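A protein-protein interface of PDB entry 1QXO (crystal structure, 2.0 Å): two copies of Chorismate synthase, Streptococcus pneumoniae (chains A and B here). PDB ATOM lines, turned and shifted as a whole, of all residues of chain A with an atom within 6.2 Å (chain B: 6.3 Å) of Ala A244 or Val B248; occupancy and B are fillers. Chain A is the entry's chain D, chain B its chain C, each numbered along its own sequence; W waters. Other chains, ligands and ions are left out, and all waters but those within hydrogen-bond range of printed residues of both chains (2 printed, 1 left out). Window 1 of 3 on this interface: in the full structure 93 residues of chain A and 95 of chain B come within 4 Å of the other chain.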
ATOM      1  N   LYS A 238      17.910   9.488  16.401  1.00  0.00           N
ATOM      2  CA  LYS A 238      17.417   8.157  16.125  1.00  0.00           C
ATOM      3  C   LYS A 238      18.314   7.500  15.087  1.00  0.00           C
ATOM      4  O   LYS A 238      18.493   8.115  14.029  1.00  0.00           O
ATOM      5  CB  LYS A 238      15.937   8.203  15.746  1.00  0.00           C
ATOM      6  CG  LYS A 238      15.080   8.607  16.970  1.00  0.00           C
ATOM      7  CD  LYS A 238      13.592   8.717  16.521  1.00  0.00           C
ATOM      8  CE  LYS A 238      12.780   9.172  17.732  1.00  0.00           C
ATOM      9  NZ  LYS A 238      11.305   9.111  17.601  1.00  0.00           N
ATOM     10  N   LEU A 239      18.901   6.370  15.397  1.00  0.00           N
ATOM     11  CA  LEU A 239      19.822   5.724  14.439  1.00  0.00           C
ATOM     12  C   LEU A 239      19.121   5.151  13.216  1.00  0.00           C
ATOM     13  O   LEU A 239      19.640   5.233  12.085  1.00  0.00           O
ATOM     14  CB  LEU A 239      20.694   4.695  15.168  1.00  0.00           C
ATOM     15  CG  LEU A 239      21.725   3.939  14.307  1.00  0.00           C
ATOM     16  CD1 LEU A 239      22.679   4.878  13.575  1.00  0.00           C
ATOM     17  CD2 LEU A 239      22.509   2.973  15.241  1.00  0.00           C
ATOM     18  N   ASP A 240      17.906   4.594  13.365  1.00  0.00           N
ATOM     19  CA  ASP A 240      17.231   4.118  12.145  1.00  0.00           C
ATOM     20  C   ASP A 240      17.027   5.271  11.167  1.00  0.00           C
ATOM     21  O   ASP A 240      17.233   5.159   9.958  1.00  0.00           O
ATOM     22  CB  ASP A 240      15.903   3.422  12.447  1.00  0.00           C
ATOM     23  CG  ASP A 240      14.979   4.131  13.411  1.00  0.00           C
ATOM     24  OD1 ASP A 240      15.259   5.187  13.984  1.00  0.00           O
ATOM     25  OD2 ASP A 240      13.827   3.683  13.645  1.00  0.00           O
ATOM     26  N   ALA A 241      16.628   6.417  11.721  1.00  0.00           N
ATOM     27  CA  ALA A 241      16.378   7.606  10.908  1.00  0.00           C
ATOM     28  C   ALA A 241      17.676   8.081  10.276  1.00  0.00           C
ATOM     29  O   ALA A 241      17.732   8.511   9.109  1.00  0.00           O
ATOM     30  CB  ALA A 241      15.757   8.753  11.786  1.00  0.00           C
ATOM     31  N   ARG A 242      18.759   8.044  11.057  1.00  0.00           N
ATOM     32  CA  ARG A 242      20.045   8.414  10.445  1.00  0.00           C
ATOM     33  C   ARG A 242      20.367   7.517   9.281  1.00  0.00           C
ATOM     34  O   ARG A 242      20.866   7.963   8.231  1.00  0.00           O
ATOM     35  CB  ARG A 242      21.184   8.374  11.509  1.00  0.00           C
ATOM     36  CG  ARG A 242      21.107   9.612  12.410  1.00  0.00           C
ATOM     37  CD  ARG A 242      22.105   9.566  13.566  1.00  0.00           C
ATOM     38  NE  ARG A 242      21.910  10.755  14.417  1.00  0.00           N
ATOM     39  CZ  ARG A 242      22.825  11.089  15.345  1.00  0.00           C
ATOM     40  NH1 ARG A 242      23.907  10.348  15.536  1.00  0.00           N
ATOM     41  NH2 ARG A 242      22.656  12.168  16.070  1.00  0.00           N
ATOM     42  N   LEU A 243      20.207   6.201   9.464  1.00  0.00           N
ATOM     43  CA  LEU A 243      20.473   5.244   8.376  1.00  0.00           C
ATOM     44  C   LEU A 243      19.538   5.522   7.194  1.00  0.00           C
ATOM     45  O   LEU A 243      19.855   5.325   6.009  1.00  0.00           O
ATOM     46  CB  LEU A 243      20.222   3.817   8.919  1.00  0.00           C
ATOM     47  CG  LEU A 243      21.293   3.221   9.859  1.00  0.00           C
ATOM     48  CD1 LEU A 243      20.826   1.941  10.518  1.00  0.00           C
ATOM     49  CD2 LEU A 243      22.561   2.831   9.087  1.00  0.00           C
ATOM     50  N   ALA A 244      18.285   5.901   7.514  1.00  0.00           N
ATOM     51  CA  ALA A 244      17.335   6.166   6.408  1.00  0.00           C
ATOM     52  C   ALA A 244      17.840   7.245   5.453  1.00  0.00           C
ATOM     53  O   ALA A 244      17.711   7.122   4.226  1.00  0.00           O
ATOM     54  CB  ALA A 244      15.961   6.540   6.939  1.00  0.00           C
ATOM     55  N   GLN A 245      18.418   8.326   6.000  1.00  0.00           N
ATOM     56  CA  GLN A 245      18.964   9.355   5.109  1.00  0.00           C
ATOM     57  C   GLN A 245      20.103   8.776   4.260  1.00  0.00           C
ATOM     58  O   GLN A 245      20.207   8.961   3.068  1.00  0.00           O
ATOM     59  CB  GLN A 245      19.545  10.538   5.909  1.00  0.00           C
ATOM     60  CG  GLN A 245      20.364  11.556   5.147  1.00  0.00           C
ATOM     61  CD  GLN A 245      20.798  12.796   5.940  1.00  0.00           C
ATOM     62  OE1 GLN A 245      20.889  13.947   5.475  1.00  0.00           O
ATOM     63  NE2 GLN A 245      21.300  12.516   7.132  1.00  0.00           N
ATOM     64  N   ALA A 246      20.992   8.036   4.928  1.00  0.00           N
ATOM     65  CA  ALA A 246      22.144   7.543   4.163  1.00  0.00           C
ATOM     66  C   ALA A 246      21.790   6.557   3.062  1.00  0.00           C
ATOM     67  O   ALA A 246      22.292   6.597   1.908  1.00  0.00           O
ATOM     68  CB  ALA A 246      23.057   6.889   5.181  1.00  0.00           C
ATOM     69  N   VAL A 247      20.792   5.729   3.312  1.00  0.00           N
ATOM     70  CA  VAL A 247      20.383   4.761   2.290  1.00  0.00           C
ATOM     71  C   VAL A 247      19.733   5.478   1.107  1.00  0.00           C
ATOM     72  O   VAL A 247      20.027   5.257  -0.092  1.00  0.00           O
ATOM     73  CB  VAL A 247      19.439   3.691   2.886  1.00  0.00           C
ATOM     74  CG1 VAL A 247      18.833   2.856   1.737  1.00  0.00           C
ATOM     75  CG2 VAL A 247      20.294   2.771   3.771  1.00  0.00           C
ATOM     76  N   VAL A 248      18.784   6.355   1.414  1.00  0.00           N
ATOM     77  CA  VAL A 248      18.068   7.056   0.361  1.00  0.00           C
ATOM     78  C   VAL A 248      18.967   8.031  -0.383  1.00  0.00           C
ATOM     79  O   VAL A 248      18.755   8.198  -1.587  1.00  0.00           O
ATOM     80  CB  VAL A 248      16.824   7.750   0.946  1.00  0.00           C
ATOM     81  CG1 VAL A 248      16.179   8.699  -0.060  1.00  0.00           C
ATOM     82  CG2 VAL A 248      15.817   6.618   1.305  1.00  0.00           C
ATOM     83  N   SER A 249      20.135   8.373   0.143  1.00  0.00           N
ATOM     84  CA  SER A 249      21.047   9.272  -0.578  1.00  0.00           C
ATOM     85  C   SER A 249      21.880   8.581  -1.669  1.00  0.00           C
ATOM     86  O   SER A 249      22.682   9.136  -2.436  1.00  0.00           O
ATOM     87  CB  SER A 249      21.988   9.861   0.501  1.00  0.00           C
ATOM     88  OG  SER A 249      22.968   8.901   0.900  1.00  0.00           O
ATOM     89  N   VAL A 256      13.500   3.212   1.809  1.00  0.00           N
ATOM     90  CA  VAL A 256      14.267   2.451   2.781  1.00  0.00           C
ATOM     91  C   VAL A 256      13.320   1.906   3.834  1.00  0.00           C
ATOM     92  O   VAL A 256      12.334   2.590   4.134  1.00  0.00           O
ATOM     93  CB  VAL A 256      15.331   3.411   3.344  1.00  0.00           C
ATOM     94  CG1 VAL A 256      14.648   4.603   4.088  1.00  0.00           C
ATOM     95  CG2 VAL A 256      16.203   2.653   4.325  1.00  0.00           C
ATOM     96  N   PHE A 258      12.835  -0.763   7.533  1.00  0.00           N
ATOM     97  CA  PHE A 258      13.473  -1.528   8.598  1.00  0.00           C
ATOM     98  C   PHE A 258      12.654  -2.738   9.061  1.00  0.00           C
ATOM     99  O   PHE A 258      11.497  -2.574   9.374  1.00  0.00           O
ATOM    100  CB  PHE A 258      13.728  -0.615   9.781  1.00  0.00           C
ATOM    101  CG  PHE A 258      14.617   0.542   9.373  1.00  0.00           C
ATOM    102  CD1 PHE A 258      14.087   1.660   8.739  1.00  0.00           C
ATOM    103  CD2 PHE A 258      15.988   0.447   9.590  1.00  0.00           C
ATOM    104  CE1 PHE A 258      14.933   2.682   8.331  1.00  0.00           C
ATOM    105  CE2 PHE A 258      16.815   1.486   9.203  1.00  0.00           C
ATOM    106  CZ  PHE A 258      16.297   2.600   8.568  1.00  0.00           C
ATOM    107  N   ALA B 241      16.684  12.449   0.695  1.00  0.00           N
ATOM    108  CA  ALA B 241      17.370  11.761   1.807  1.00  0.00           C
ATOM    109  C   ALA B 241      17.164  12.478   3.123  1.00  0.00           C
ATOM    110  O   ALA B 241      16.910  11.820   4.146  1.00  0.00           O
ATOM    111  CB  ALA B 241      18.826  11.550   1.492  1.00  0.00           C
ATOM    112  N   LEU B 243      14.479  14.181   3.851  1.00  0.00           N
ATOM    113  CA  LEU B 243      13.112  13.867   4.238  1.00  0.00           C
ATOM    114  C   LEU B 243      13.019  12.460   4.827  1.00  0.00           C
ATOM    115  O   LEU B 243      12.253  12.215   5.740  1.00  0.00           O
ATOM    116  CB  LEU B 243      12.136  13.916   3.036  1.00  0.00           C
ATOM    117  CG  LEU B 243      11.920  15.417   2.631  1.00  0.00           C
ATOM    118  CD1 LEU B 243      11.482  15.547   1.190  1.00  0.00           C
ATOM    119  CD2 LEU B 243      10.924  16.029   3.565  1.00  0.00           C
ATOM    120  N   ALA B 244      13.813  11.557   4.247  1.00  0.00           N
ATOM    121  CA  ALA B 244      13.817  10.184   4.712  1.00  0.00           C
ATOM    122  C   ALA B 244      14.162  10.135   6.183  1.00  0.00           C
ATOM    123  O   ALA B 244      13.502   9.434   7.009  1.00  0.00           O
ATOM    124  CB  ALA B 244      14.687   9.323   3.794  1.00  0.00           C
ATOM    125  N   GLN B 245      15.218  10.828   6.580  1.00  0.00           N
ATOM    126  CA  GLN B 245      15.584  10.802   7.994  1.00  0.00           C
ATOM    127  C   GLN B 245      14.406  11.343   8.799  1.00  0.00           C
ATOM    128  O   GLN B 245      13.926  10.722   9.767  1.00  0.00           O
ATOM    129  CB  GLN B 245      16.848  11.674   8.285  1.00  0.00           C
ATOM    130  CG  GLN B 245      17.064  11.833   9.778  1.00  0.00           C
ATOM    131  CD  GLN B 245      18.267  12.702  10.145  1.00  0.00           C
ATOM    132  OE1 GLN B 245      18.979  12.432  11.140  1.00  0.00           O
ATOM    133  NE2 GLN B 245      18.537  13.754   9.405  1.00  0.00           N
ATOM    134  N   ALA B 246      13.884  12.508   8.430  1.00  0.00           N
ATOM    135  CA  ALA B 246      12.775  13.060   9.204  1.00  0.00           C
ATOM    136  C   ALA B 246      11.543  12.162   9.314  1.00  0.00           C
ATOM    137  O   ALA B 246      10.955  12.031  10.409  1.00  0.00           O
ATOM    138  CB  ALA B 246      12.429  14.450   8.642  1.00  0.00           C
ATOM    139  N   VAL B 247      11.168  11.458   8.227  1.00  0.00           N
ATOM    140  CA  VAL B 247       9.970  10.615   8.282  1.00  0.00           C
ATOM    141  C   VAL B 247      10.199   9.409   9.190  1.00  0.00           C
ATOM    142  O   VAL B 247       9.339   9.055   9.999  1.00  0.00           O
ATOM    143  CB  VAL B 247       9.490  10.146   6.882  1.00  0.00           C
ATOM    144  CG1 VAL B 247       8.325   9.141   6.949  1.00  0.00           C
ATOM    145  CG2 VAL B 247       9.013  11.341   6.065  1.00  0.00           C
ATOM    146  N   VAL B 248      11.325   8.716   9.024  1.00  0.00           N
ATOM    147  CA  VAL B 248      11.569   7.551   9.852  1.00  0.00           C
ATOM    148  C   VAL B 248      11.810   7.957  11.285  1.00  0.00           C
ATOM    149  O   VAL B 248      11.578   7.065  12.075  1.00  0.00           O
ATOM    150  CB  VAL B 248      12.755   6.730   9.277  1.00  0.00           C
ATOM    151  CG1 VAL B 248      13.252   5.626  10.215  1.00  0.00           C
ATOM    152  CG2 VAL B 248      12.340   6.142   7.924  1.00  0.00           C
ATOM    153  N   SER B 249      12.220   9.190  11.592  1.00  0.00           N
ATOM    154  CA  SER B 249      12.334   9.659  12.950  1.00  0.00           C
ATOM    155  C   SER B 249      10.984   9.760  13.693  1.00  0.00           C
ATOM    156  O   SER B 249      10.992   9.872  14.937  1.00  0.00           O
ATOM    157  CB  SER B 249      12.995  11.028  13.048  1.00  0.00           C
ATOM    158  OG  SER B 249      12.060  12.129  12.787  1.00  0.00           O
ATOM    159  N   ILE B 250       9.880   9.662  12.950  1.00  0.00           N
ATOM    160  CA  ILE B 250       8.583   9.741  13.661  1.00  0.00           C
ATOM    161  C   ILE B 250       8.365   8.457  14.444  1.00  0.00           C
ATOM    162  O   ILE B 250       8.583   7.381  13.893  1.00  0.00           O
ATOM    163  CB  ILE B 250       7.394   9.969  12.708  1.00  0.00           C
ATOM    164  CG1 ILE B 250       7.600  11.290  11.947  1.00  0.00           C
ATOM    165  CG2 ILE B 250       6.100  10.028  13.523  1.00  0.00           C
ATOM    166  CD1 ILE B 250       6.752  11.373  10.676  1.00  0.00           C
ATOM    167  N   ASN B 251       7.942   8.544  15.691  1.00  0.00           N
ATOM    168  CA  ASN B 251       7.614   7.361  16.479  1.00  0.00           C
ATOM    169  C   ASN B 251       6.802   6.327  15.708  1.00  0.00           C
ATOM    170  O   ASN B 251       5.769   6.701  15.142  1.00  0.00           O
ATOM    171  CB  ASN B 251       6.678   7.811  17.623  1.00  0.00           C
ATOM    172  CG  ASN B 251       7.481   8.630  18.634  1.00  0.00           C
ATOM    173  OD1 ASN B 251       8.173   9.575  18.293  1.00  0.00           O
ATOM    174  ND2 ASN B 251       7.372   8.261  19.886  1.00  0.00           N
ATOM    175  N   ALA B 252       7.299   5.077  15.704  1.00  0.00           N
ATOM    176  CA  ALA B 252       6.577   3.961  15.110  1.00  0.00           C
ATOM    177  C   ALA B 252       6.752   3.852  13.614  1.00  0.00           C
ATOM    178  O   ALA B 252       6.320   2.833  13.055  1.00  0.00           O
ATOM    179  CB  ALA B 252       5.091   3.889  15.512  1.00  0.00           C
ATOM    180  N   PHE B 253       7.460   4.798  12.957  1.00  0.00           N
ATOM    181  CA  PHE B 253       7.677   4.653  11.528  1.00  0.00           C
ATOM    182  C   PHE B 253       8.850   3.696  11.272  1.00  0.00           C
ATOM    183  O   PHE B 253       9.963   3.714  11.825  1.00  0.00           O
ATOM    184  CB  PHE B 253       7.811   5.975  10.779  1.00  0.00           C
ATOM    185  CG  PHE B 253       6.515   6.747  10.593  1.00  0.00           C
ATOM    186  CD1 PHE B 253       5.676   7.048  11.631  1.00  0.00           C
ATOM    187  CD2 PHE B 253       6.155   7.187   9.311  1.00  0.00           C
ATOM    188  CE1 PHE B 253       4.502   7.776  11.433  1.00  0.00           C
ATOM    189  CE2 PHE B 253       5.004   7.899   9.088  1.00  0.00           C
ATOM    190  CZ  PHE B 253       4.149   8.196  10.149  1.00  0.00           C
ATOM    191  N   LYS B 254       8.638   2.780  10.351  1.00  0.00           N
ATOM    192  CA  LYS B 254       9.669   1.753  10.044  1.00  0.00           C
ATOM    193  C   LYS B 254      10.106   1.845   8.609  1.00  0.00           C
ATOM    194  O   LYS B 254      10.787   0.958   8.068  1.00  0.00           O
ATOM    195  CB  LYS B 254       9.020   0.352  10.344  1.00  0.00           C
ATOM    196  CG  LYS B 254       8.685   0.234  11.836  1.00  0.00           C
ATOM    197  CD  LYS B 254       9.901   0.304  12.773  1.00  0.00           C
ATOM    198  CE  LYS B 254      10.775  -0.929  12.610  1.00  0.00           C
ATOM    199  NZ  LYS B 254      11.882  -0.939  13.604  1.00  0.00           N
ATOM    200  N   GLY B 255       9.684   2.873   7.897  1.00  0.00           N
ATOM    201  CA  GLY B 255      10.063   2.999   6.497  1.00  0.00           C
ATOM    202  C   GLY B 255       9.567   4.280   5.839  1.00  0.00           C
ATOM    203  O   GLY B 255       8.602   4.905   6.287  1.00  0.00           O
ATOM    204  N   VAL B 256      10.207   4.572   4.695  1.00  0.00           N
ATOM    205  CA  VAL B 256       9.796   5.756   3.920  1.00  0.00           C
ATOM    206  C   VAL B 256      10.059   5.522   2.443  1.00  0.00           C
ATOM    207  O   VAL B 256      10.990   4.782   2.088  1.00  0.00           O
ATOM    208  CB  VAL B 256      10.484   7.025   4.494  1.00  0.00           C
ATOM    209  CG1 VAL B 256      11.981   6.808   4.312  1.00  0.00           C
ATOM    210  CG2 VAL B 256       9.946   8.266   3.730  1.00  0.00           C
HETATM  211  O   HOH W   1      17.632  10.868  13.386  1.00  0.00           O
HETATM  212  O   HOH W   2      13.292   1.379  12.480  1.00  0.00           O
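OG of Ser B249 sits at hydrogen-bond distance from O of Ala B246, at 2.6 Å.
OG of Ser A249 is in hydrogen-bond range of O of Ala A246 (2.6 Å).
Among the printed residues, pairs that only touch across the chains: Val A256 with Gly B255, Gln A245 with Ala B241, Ala A241 with Gln B245, Ala A241 with Ser B249, Ser A249 with Ala B241, Arg A242 with Gln B245, Ala A241 with Val B248, Ala A244 with Ala B244, Gln A245 with Gln B245, Ala A244 with Val B248, Val A248 with Ala B241, Val A248 with Ala B244, Phe A258 with Val B248 and Asp A240 with Val B248.
O of Ser B249 sits at hydrogen-bond distance from NZ of Lys A238.
The side-chain amino group (NZ) of Lys A238 sits at hydrogen-bond distance from the side-chain amide oxygen (OD1) of Asn B251 (3.2 Å).
O of Lys B254 sits at hydrogen-bond distance from N of Phe A258.
N of Val B256 lies within hydrogen-bond range of O of Val A256 (3.0 Å).
Ala A244 touches just these residues of chain B: Ala B244 and Val B248.
Of the printed residues of chain B, Val A248 touches Ala B241 (3.8 Å) and Ala B244 (3.8 Å).
Val B248 touches four residues of chain A.
Printed residues of chain A within 4 Å of Ser B249: Lys A238 (2.8 Å) and Ala A241 (3.6 Å).
The nearest printed residue of chain A that does not touch Gly B255 is Phe A258 (4.6 Å).
Water W2 bridges the side-chain carboxylate of Asp A240 (2.6 Å) and the side-chain amino group of Lys B254 (2.9 Å).
Water W1 bridges the backbone carbonyl oxygen (O) of Lys A238 (3.0 Å) and the side-chain amide oxygen (OE1) of Gln B245 (3.1 Å).
Ala A241 touches Gln B245, and with the chains exchanged Gln A245 touches Ala B241.
Ala A241 touches Val B248, and with the chains exchanged Val A248 touches Ala B241.
Ala B244 touches its own counterpart, Ala A244.
Val B256 touches its own counterpart, Val A256.
Of the 15 printed residues of chain B, 9 touch a printed residue of chain A.
Hydrophobic or aromatic side chains of chain B that line the printed part of chain A: Ala B241, Ala B244, Val B248 and Val B256.
Along chain B the printed residues that touch a printed residue of chain A span positions 241 to 256.
Among the printed residues, 18 pairs touch across the chains.
Among the printed residues, no Asp or Glu carboxylate lies within 4 Å of a Lys or Arg side-chain nitrogen of the other chain.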
